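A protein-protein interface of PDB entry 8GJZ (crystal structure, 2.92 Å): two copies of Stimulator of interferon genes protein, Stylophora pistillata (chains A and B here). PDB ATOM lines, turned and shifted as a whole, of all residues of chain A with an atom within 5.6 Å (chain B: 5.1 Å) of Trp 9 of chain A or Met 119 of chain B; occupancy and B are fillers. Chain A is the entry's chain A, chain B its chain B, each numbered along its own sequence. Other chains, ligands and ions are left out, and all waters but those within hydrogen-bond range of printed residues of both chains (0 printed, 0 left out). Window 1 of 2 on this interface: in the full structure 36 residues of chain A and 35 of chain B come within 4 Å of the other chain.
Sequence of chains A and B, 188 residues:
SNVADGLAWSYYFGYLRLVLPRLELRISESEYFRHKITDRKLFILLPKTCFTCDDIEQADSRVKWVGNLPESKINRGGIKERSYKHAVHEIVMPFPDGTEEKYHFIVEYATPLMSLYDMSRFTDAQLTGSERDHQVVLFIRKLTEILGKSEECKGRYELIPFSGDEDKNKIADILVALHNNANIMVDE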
ATOM      1  N   ALA A   4     -22.523  -9.816  -8.389  1.00  0.00           N
ATOM      2  CA  ALA A   4     -22.173 -11.222  -8.228  1.00  0.00           C
ATOM      3  C   ALA A   4     -21.569 -11.807  -9.498  1.00  0.00           C
ATOM      4  O   ALA A   4     -20.714 -12.697  -9.419  1.00  0.00           O
ATOM      5  CB  ALA A   4     -23.403 -12.025  -7.808  1.00  0.00           C
ATOM      6  N   ASP A   5     -21.997 -11.328 -10.671  1.00  0.00           N
ATOM      7  CA  ASP A   5     -21.461 -11.852 -11.925  1.00  0.00           C
ATOM      8  C   ASP A   5     -19.952 -11.663 -12.001  1.00  0.00           C
ATOM      9  O   ASP A   5     -19.225 -12.568 -12.429  1.00  0.00           O
ATOM     10  CB  ASP A   5     -22.144 -11.179 -13.115  1.00  0.00           C
ATOM     11  CG  ASP A   5     -23.601 -11.581 -13.258  1.00  0.00           C
ATOM     12  OD1 ASP A   5     -24.049 -12.482 -12.517  1.00  0.00           O
ATOM     13  OD2 ASP A   5     -24.298 -10.995 -14.113  1.00  0.00           O
ATOM     14  N   GLY A   6     -19.460 -10.496 -11.585  1.00  0.00           N
ATOM     15  CA  GLY A   6     -18.025 -10.280 -11.566  1.00  0.00           C
ATOM     16  C   GLY A   6     -17.313 -11.174 -10.569  1.00  0.00           C
ATOM     17  O   GLY A   6     -16.234 -11.700 -10.855  1.00  0.00           O
ATOM     18  N   LEU A   7     -17.908 -11.365  -9.390  1.00  0.00           N
ATOM     19  CA  LEU A   7     -17.259 -12.177  -8.366  1.00  0.00           C
ATOM     20  C   LEU A   7     -17.214 -13.645  -8.768  1.00  0.00           C
ATOM     21  O   LEU A   7     -16.205 -14.323  -8.545  1.00  0.00           O
ATOM     22  CB  LEU A   7     -17.974 -12.008  -7.027  1.00  0.00           C
ATOM     23  CG  LEU A   7     -18.020 -10.589  -6.459  1.00  0.00           C
ATOM     24  CD1 LEU A   7     -18.584 -10.610  -5.052  1.00  0.00           C
ATOM     25  CD2 LEU A   7     -16.641  -9.948  -6.480  1.00  0.00           C
ATOM     26  N   ALA A   8     -18.295 -14.153  -9.362  1.00  0.00           N
ATOM     27  CA  ALA A   8     -18.312 -15.550  -9.783  1.00  0.00           C
ATOM     28  C   ALA A   8     -17.346 -15.790 -10.937  1.00  0.00           C
ATOM     29  O   ALA A   8     -16.644 -16.808 -10.963  1.00  0.00           O
ATOM     30  CB  ALA A   8     -19.731 -15.969 -10.169  1.00  0.00           C
ATOM     31  N   TRP A   9     -17.292 -14.865 -11.898  1.00  0.00           N
ATOM     32  CA  TRP A   9     -16.363 -15.024 -13.013  1.00  0.00           C
ATOM     33  C   TRP A   9     -14.920 -14.844 -12.561  1.00  0.00           C
ATOM     34  O   TRP A   9     -14.024 -15.556 -13.032  1.00  0.00           O
ATOM     35  CB  TRP A   9     -16.707 -14.046 -14.135  1.00  0.00           C
ATOM     36  CG  TRP A   9     -17.856 -14.493 -14.993  1.00  0.00           C
ATOM     37  CD1 TRP A   9     -19.065 -13.877 -15.134  1.00  0.00           C
ATOM     38  CD2 TRP A   9     -17.904 -15.662 -15.822  1.00  0.00           C
ATOM     39  NE1 TRP A   9     -19.860 -14.587 -16.002  1.00  0.00           N
ATOM     40  CE2 TRP A   9     -19.170 -15.686 -16.437  1.00  0.00           C
ATOM     41  CE3 TRP A   9     -16.998 -16.689 -16.103  1.00  0.00           C
ATOM     42  CZ2 TRP A   9     -19.551 -16.696 -17.318  1.00  0.00           C
ATOM     43  CZ3 TRP A   9     -17.378 -17.690 -16.978  1.00  0.00           C
ATOM     44  CH2 TRP A   9     -18.644 -17.686 -17.574  1.00  0.00           C
ATOM     45  N   SER A  10     -14.670 -13.898 -11.652  1.00  0.00           N
ATOM     46  CA  SER A  10     -13.330 -13.760 -11.090  1.00  0.00           C
ATOM     47  C   SER A  10     -12.925 -15.019 -10.336  1.00  0.00           C
ATOM     48  O   SER A  10     -11.783 -15.479 -10.448  1.00  0.00           O
ATOM     49  CB  SER A  10     -13.269 -12.538 -10.174  1.00  0.00           C
ATOM     50  OG  SER A  10     -11.992 -12.415  -9.570  1.00  0.00           O
ATOM     51  N   TYR A  11     -13.857 -15.596  -9.573  1.00  0.00           N
ATOM     52  CA  TYR A  11     -13.578 -16.827  -8.837  1.00  0.00           C
ATOM     53  C   TYR A  11     -13.239 -17.972  -9.785  1.00  0.00           C
ATOM     54  O   TYR A  11     -12.395 -18.820  -9.472  1.00  0.00           O
ATOM     55  CB  TYR A  11     -14.784 -17.183  -7.964  1.00  0.00           C
ATOM     56  CG  TYR A  11     -14.553 -18.285  -6.953  1.00  0.00           C
ATOM     57  CD1 TYR A  11     -13.415 -18.303  -6.161  1.00  0.00           C
ATOM     58  CD2 TYR A  11     -15.494 -19.289  -6.768  1.00  0.00           C
ATOM     59  CE1 TYR A  11     -13.209 -19.303  -5.228  1.00  0.00           C
ATOM     60  CE2 TYR A  11     -15.298 -20.292  -5.837  1.00  0.00           C
ATOM     61  CZ  TYR A  11     -14.154 -20.294  -5.069  1.00  0.00           C
ATOM     62  OH  TYR A  11     -13.952 -21.289  -4.139  1.00  0.00           O
ATOM     63  N   TYR A  12     -13.878 -18.004 -10.954  1.00  0.00           N
ATOM     64  CA  TYR A  12     -13.631 -19.074 -11.913  1.00  0.00           C
ATOM     65  C   TYR A  12     -12.342 -18.843 -12.693  1.00  0.00           C
ATOM     66  O   TYR A  12     -11.466 -19.716 -12.727  1.00  0.00           O
ATOM     67  CB  TYR A  12     -14.826 -19.201 -12.861  1.00  0.00           C
ATOM     68  CG  TYR A  12     -14.614 -20.146 -14.022  1.00  0.00           C
ATOM     69  CD1 TYR A  12     -14.758 -21.518 -13.864  1.00  0.00           C
ATOM     70  CD2 TYR A  12     -14.287 -19.664 -15.284  1.00  0.00           C
ATOM     71  CE1 TYR A  12     -14.571 -22.384 -14.926  1.00  0.00           C
ATOM     72  CE2 TYR A  12     -14.099 -20.519 -16.350  1.00  0.00           C
ATOM     73  CZ  TYR A  12     -14.242 -21.878 -16.167  1.00  0.00           C
ATOM     74  OH  TYR A  12     -14.055 -22.732 -17.229  1.00  0.00           O
ATOM     75  N   PHE A  13     -12.200 -17.668 -13.314  1.00  0.00           N
ATOM     76  CA  PHE A  13     -11.054 -17.420 -14.188  1.00  0.00           C
ATOM     77  C   PHE A  13      -9.750 -17.343 -13.404  1.00  0.00           C
ATOM     78  O   PHE A  13      -8.716 -17.843 -13.862  1.00  0.00           O
ATOM     79  CB  PHE A  13     -11.265 -16.135 -14.985  1.00  0.00           C
ATOM     80  CG  PHE A  13     -12.122 -16.312 -16.197  1.00  0.00           C
ATOM     81  CD1 PHE A  13     -11.756 -17.204 -17.191  1.00  0.00           C
ATOM     82  CD2 PHE A  13     -13.289 -15.585 -16.351  1.00  0.00           C
ATOM     83  CE1 PHE A  13     -12.540 -17.373 -18.311  1.00  0.00           C
ATOM     84  CE2 PHE A  13     -14.077 -15.748 -17.470  1.00  0.00           C
ATOM     85  CZ  PHE A  13     -13.703 -16.645 -18.451  1.00  0.00           C
ATOM     86  N   GLY A  14      -9.772 -16.713 -12.237  1.00  0.00           N
ATOM     87  CA  GLY A  14      -8.565 -16.531 -11.465  1.00  0.00           C
ATOM     88  C   GLY A  14      -8.206 -17.651 -10.520  1.00  0.00           C
ATOM     89  O   GLY A  14      -7.159 -17.576  -9.869  1.00  0.00           O
ATOM     90  N   LYS A 142     -25.031 -18.256 -10.138  1.00  0.00           N
ATOM     91  CA  LYS A 142     -24.130 -18.000 -11.257  1.00  0.00           C
ATOM     92  C   LYS A 142     -22.938 -18.947 -11.237  1.00  0.00           C
ATOM     93  O   LYS A 142     -22.537 -19.469 -12.283  1.00  0.00           O
ATOM     94  CB  LYS A 142     -23.654 -16.549 -11.235  1.00  0.00           C
ATOM     95  CG  LYS A 142     -22.832 -16.169 -12.450  1.00  0.00           C
ATOM     96  CD  LYS A 142     -23.630 -16.391 -13.722  1.00  0.00           C
ATOM     97  CE  LYS A 142     -22.748 -16.322 -14.952  1.00  0.00           C
ATOM     98  NZ  LYS A 142     -23.544 -16.458 -16.205  1.00  0.00           N
ATOM     99  N   ILE A 146     -21.711 -21.528 -14.255  1.00  0.00           N
ATOM    100  CA  ILE A 146     -20.383 -21.467 -14.855  1.00  0.00           C
ATOM    101  C   ILE A 146     -19.699 -22.825 -14.773  1.00  0.00           C
ATOM    102  O   ILE A 146     -19.181 -23.341 -15.771  1.00  0.00           O
ATOM    103  CB  ILE A 146     -19.541 -20.367 -14.186  1.00  0.00           C
ATOM    104  CG1 ILE A 146     -20.176 -18.995 -14.423  1.00  0.00           C
ATOM    105  CG2 ILE A 146     -18.115 -20.394 -14.708  1.00  0.00           C
ATOM    106  CD1 ILE A 146     -19.495 -17.872 -13.672  1.00  0.00           C
ATOM    107  N   VAL B   3     -20.645  -4.726 -12.854  1.00  0.00           N
ATOM    108  CA  VAL B   3     -19.591  -5.733 -12.765  1.00  0.00           C
ATOM    109  C   VAL B   3     -18.317  -5.114 -12.210  1.00  0.00           C
ATOM    110  O   VAL B   3     -17.642  -5.701 -11.355  1.00  0.00           O
ATOM    111  CB  VAL B   3     -19.345  -6.372 -14.144  1.00  0.00           C
ATOM    112  CG1 VAL B   3     -18.525  -7.644 -14.001  1.00  0.00           C
ATOM    113  CG2 VAL B   3     -20.659  -6.640 -14.851  1.00  0.00           C
ATOM    114  N   LEU B   7     -15.826  -5.927  -8.700  1.00  0.00           N
ATOM    115  CA  LEU B   7     -14.409  -6.253  -8.814  1.00  0.00           C
ATOM    116  C   LEU B   7     -13.537  -5.230  -8.100  1.00  0.00           C
ATOM    117  O   LEU B   7     -12.500  -5.590  -7.531  1.00  0.00           O
ATOM    118  CB  LEU B   7     -14.009  -6.356 -10.285  1.00  0.00           C
ATOM    119  CG  LEU B   7     -14.685  -7.459 -11.095  1.00  0.00           C
ATOM    120  CD1 LEU B   7     -14.141  -7.480 -12.513  1.00  0.00           C
ATOM    121  CD2 LEU B   7     -14.495  -8.810 -10.423  1.00  0.00           C
ATOM    122  N   SER B 115      -9.584 -10.523 -15.417  1.00  0.00           N
ATOM    123  CA  SER B 115     -10.836 -11.274 -15.388  1.00  0.00           C
ATOM    124  C   SER B 115     -11.871 -10.658 -16.322  1.00  0.00           C
ATOM    125  O   SER B 115     -12.655 -11.382 -16.947  1.00  0.00           O
ATOM    126  CB  SER B 115     -11.375 -11.351 -13.959  1.00  0.00           C
ATOM    127  OG  SER B 115     -10.548 -12.161 -13.143  1.00  0.00           O
ATOM    128  N   LEU B 116     -11.889  -9.326 -16.432  1.00  0.00           N
ATOM    129  CA  LEU B 116     -12.799  -8.676 -17.371  1.00  0.00           C
ATOM    130  C   LEU B 116     -12.489  -9.082 -18.805  1.00  0.00           C
ATOM    131  O   LEU B 116     -13.403  -9.349 -19.594  1.00  0.00           O
ATOM    132  CB  LEU B 116     -12.722  -7.157 -17.218  1.00  0.00           C
ATOM    133  CG  LEU B 116     -13.461  -6.552 -16.025  1.00  0.00           C
ATOM    134  CD1 LEU B 116     -13.247  -5.047 -15.970  1.00  0.00           C
ATOM    135  CD2 LEU B 116     -14.942  -6.882 -16.099  1.00  0.00           C
ATOM    136  N   TYR B 117     -11.203  -9.132 -19.162  1.00  0.00           N
ATOM    137  CA  TYR B 117     -10.830  -9.583 -20.497  1.00  0.00           C
ATOM    138  C   TYR B 117     -11.198 -11.046 -20.705  1.00  0.00           C
ATOM    139  O   TYR B 117     -11.663 -11.430 -21.784  1.00  0.00           O
ATOM    140  CB  TYR B 117      -9.336  -9.366 -20.728  1.00  0.00           C
ATOM    141  CG  TYR B 117      -8.829  -9.962 -22.021  1.00  0.00           C
ATOM    142  CD1 TYR B 117      -9.171  -9.406 -23.247  1.00  0.00           C
ATOM    143  CD2 TYR B 117      -8.004 -11.080 -22.017  1.00  0.00           C
ATOM    144  CE1 TYR B 117      -8.712  -9.949 -24.432  1.00  0.00           C
ATOM    145  CE2 TYR B 117      -7.538 -11.629 -23.197  1.00  0.00           C
ATOM    146  CZ  TYR B 117      -7.895 -11.060 -24.402  1.00  0.00           C
ATOM    147  OH  TYR B 117      -7.436 -11.600 -25.581  1.00  0.00           O
ATOM    148  N   ASP B 118     -11.004 -11.877 -19.678  1.00  0.00           N
ATOM    149  CA  ASP B 118     -11.341 -13.291 -19.797  1.00  0.00           C
ATOM    150  C   ASP B 118     -12.837 -13.503 -19.983  1.00  0.00           C
ATOM    151  O   ASP B 118     -13.245 -14.465 -20.643  1.00  0.00           O
ATOM    152  CB  ASP B 118     -10.846 -14.057 -18.571  1.00  0.00           C
ATOM    153  CG  ASP B 118      -9.334 -14.155 -18.518  1.00  0.00           C
ATOM    154  OD1 ASP B 118      -8.700 -14.187 -19.594  1.00  0.00           O
ATOM    155  OD2 ASP B 118      -8.780 -14.205 -17.398  1.00  0.00           O
ATOM    156  N   MET B 119     -13.666 -12.624 -19.415  1.00  0.00           N
ATOM    157  CA  MET B 119     -15.109 -12.755 -19.583  1.00  0.00           C
ATOM    158  C   MET B 119     -15.498 -12.632 -21.052  1.00  0.00           C
ATOM    159  O   MET B 119     -16.123 -13.533 -21.620  1.00  0.00           O
ATOM    160  CB  MET B 119     -15.842 -11.703 -18.747  1.00  0.00           C
ATOM    161  CG  MET B 119     -15.713 -11.883 -17.243  1.00  0.00           C
ATOM    162  SD  MET B 119     -16.828 -10.803 -16.321  1.00  0.00           S
ATOM    163  CE  MET B 119     -15.895 -10.553 -14.813  1.00  0.00           C
ATOM    164  N   SER B 120     -15.118 -11.523 -21.686  1.00  0.00           N
ATOM    165  CA  SER B 120     -15.517 -11.256 -23.063  1.00  0.00           C
ATOM    166  C   SER B 120     -14.783 -12.118 -24.081  1.00  0.00           C
ATOM    167  O   SER B 120     -15.213 -12.175 -25.238  1.00  0.00           O
ATOM    168  CB  SER B 120     -15.286  -9.783 -23.395  1.00  0.00           C
ATOM    169  OG  SER B 120     -13.905  -9.472 -23.351  1.00  0.00           O
ATOM    170  N   ARG B 121     -13.699 -12.788 -23.688  1.00  0.00           N
ATOM    171  CA  ARG B 121     -12.871 -13.495 -24.660  1.00  0.00           C
ATOM    172  C   ARG B 121     -13.537 -14.783 -25.128  1.00  0.00           C
ATOM    173  O   ARG B 121     -13.800 -14.963 -26.324  1.00  0.00           O
ATOM    174  CB  ARG B 121     -11.494 -13.782 -24.062  1.00  0.00           C
ATOM    175  CG  ARG B 121     -10.545 -14.489 -25.016  1.00  0.00           C
ATOM    176  CD  ARG B 121      -9.156 -14.612 -24.419  1.00  0.00           C
ATOM    177  NE  ARG B 121      -9.157 -15.387 -23.183  1.00  0.00           N
ATOM    178  CZ  ARG B 121      -8.101 -15.536 -22.396  1.00  0.00           C
ATOM    179  NH1 ARG B 121      -6.940 -14.968 -22.679  1.00  0.00           N
ATOM    180  NH2 ARG B 121      -8.213 -16.271 -21.293  1.00  0.00           N
ATOM    181  N   PHE B 122     -13.812 -15.696 -24.201  1.00  0.00           N
ATOM    182  CA  PHE B 122     -14.322 -17.006 -24.574  1.00  0.00           C
ATOM    183  C   PHE B 122     -15.754 -16.912 -25.098  1.00  0.00           C
ATOM    184  O   PHE B 122     -16.447 -15.907 -24.921  1.00  0.00           O
ATOM    185  CB  PHE B 122     -14.259 -17.965 -23.385  1.00  0.00           C
ATOM    186  CG  PHE B 122     -12.862 -18.261 -22.922  1.00  0.00           C
ATOM    187  CD1 PHE B 122     -12.112 -19.255 -23.532  1.00  0.00           C
ATOM    188  CD2 PHE B 122     -12.296 -17.545 -21.880  1.00  0.00           C
ATOM    189  CE1 PHE B 122     -10.824 -19.529 -23.110  1.00  0.00           C
ATOM    190  CE2 PHE B 122     -11.009 -17.814 -21.453  1.00  0.00           C
ATOM    191  CZ  PHE B 122     -10.272 -18.808 -22.069  1.00  0.00           C
ATOM    192  N   ALA B 125     -19.881 -15.441 -24.000  1.00  0.00           N
ATOM    193  CA  ALA B 125     -19.400 -14.418 -23.086  1.00  0.00           C
ATOM    194  C   ALA B 125     -20.550 -13.545 -22.606  1.00  0.00           C
ATOM    195  O   ALA B 125     -21.440 -13.176 -23.379  1.00  0.00           O
ATOM    196  CB  ALA B 125     -18.341 -13.555 -23.769  1.00  0.00           C
ATOM    197  N   GLN B 126     -20.534 -13.217 -21.313  1.00  0.00           N
ATOM    198  CA  GLN B 126     -21.512 -12.269 -20.795  1.00  0.00           C
ATOM    199  C   GLN B 126     -21.232 -10.861 -21.303  1.00  0.00           C
ATOM    200  O   GLN B 126     -22.160 -10.133 -21.674  1.00  0.00           O
ATOM    201  CB  GLN B 126     -21.520 -12.297 -19.267  1.00  0.00           C
ATOM    202  CG  GLN B 126     -22.120 -13.557 -18.678  1.00  0.00           C
ATOM    203  CD  GLN B 126     -22.740 -13.316 -17.319  1.00  0.00           C
ATOM    204  OE1 GLN B 126     -23.651 -14.033 -16.903  1.00  0.00           O
ATOM    205  NE2 GLN B 126     -22.252 -12.297 -16.620  1.00  0.00           N
ATOM    206  N   LEU B 127     -19.962 -10.467 -21.336  1.00  0.00           N
ATOM    207  CA  LEU B 127     -19.573  -9.145 -21.800  1.00  0.00           C
ATOM    208  C   LEU B 127     -19.202  -9.184 -23.275  1.00  0.00           C
ATOM    209  O   LEU B 127     -18.554 -10.124 -23.744  1.00  0.00           O
ATOM    210  CB  LEU B 127     -18.391  -8.612 -20.989  1.00  0.00           C
ATOM    211  CG  LEU B 127     -18.649  -8.293 -19.518  1.00  0.00           C
ATOM    212  CD1 LEU B 127     -17.363  -7.846 -18.849  1.00  0.00           C
ATOM    213  CD2 LEU B 127     -19.726  -7.226 -19.382  1.00  0.00           C
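The side-chain carboxylate of Asp 118 of chain B is in salt-bridge range of the guanidinium group of Arg 121 of chain B.
Gly 6 of chain A touches Val 3 of chain B. Leu 7 of chain B touches Gly 6 of chain A. CA of Gly 6 of chain A touches CE of Met 119 of chain B, at 3.9 Å. CB of Trp 9 of chain A touches CE of Met 119 of chain B, at 3.6 Å. Ser 10 of chain A touches Leu 7 of chain B. Ser 10 of chain A touches Ser 115 of chain B. Phe 13 of chain A touches Asp 118 of chain B (CZ to O, 3.1 Å). Met 119 of chain B touches Phe 13 of chain A (N to CE2, 3.7 Å). Phe 13 of chain A touches Phe 122 of chain B.
The side-chain amino group of Lys 142 of chain A lies within hydrogen-bond range of the side-chain amide oxygen of Gln 126 of chain B, 2.5 Å away. The indole nitrogen (NE1) of Trp 9 of chain A sits close to the side-chain amide nitrogen (NE2) of Gln 126 of chain B (3.4 Å). The side-chain amide nitrogen (NE2) of Gln 126 of chain B sits at hydrogen-bond distance from the side-chain carboxylate (OD2) of Asp 5 of chain A, 3.5 Å away.
Of the 13 printed residues of chain B, 7 touch a printed residue of chain A. Of the 13 printed residues of chain A, 6 touch a printed residue of chain B. Printed residues of chain A that touch a printed residue of chain B: Asp 5, Gly 6, Trp 9, Ser 10, Phe 13 and Lys 142. Among the printed residues, no Asp or Glu carboxylate lies within 4 Å of a Lys or Arg side-chain nitrogen of the other chain.
Position printed for both chains: 7.
Trp 9 of chain A touches two residues of chain B. Met 119 of chain B touches just these residues of chain A: Gly 6, Trp 9 and Phe 13. Printed residues of chain B within 4 Å of Asp 5 of chain A: Gln 126 (3.5 Å). Of the printed residues of chain A, Gln 126 of chain B touches Asp 5 (3.5 Å), Trp 9 (3.4 Å) and Lys 142 (2.5 Å). Of the printed residues of chain A, Phe 122 of chain B touches Phe 13. Of the printed residues of chain B, Ser 10 of chain A touches Leu 7 and Ser 115. Printed residues of chain A within 4 Å of Leu 7 of chain B: Gly 6 and Ser 10. Gly 14 of chain A touches none of the printed residues of chain B. Leu 127 of chain B touches none of the printed residues of chain A. The nearest residue of chain B that does not touch Trp 9 of chain A is Ser 115 of chain B (4.9 Å). The nearest printed residue of chain B that does not touch Phe 13 of chain A is Ser 115 of chain B (4.3 Å).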
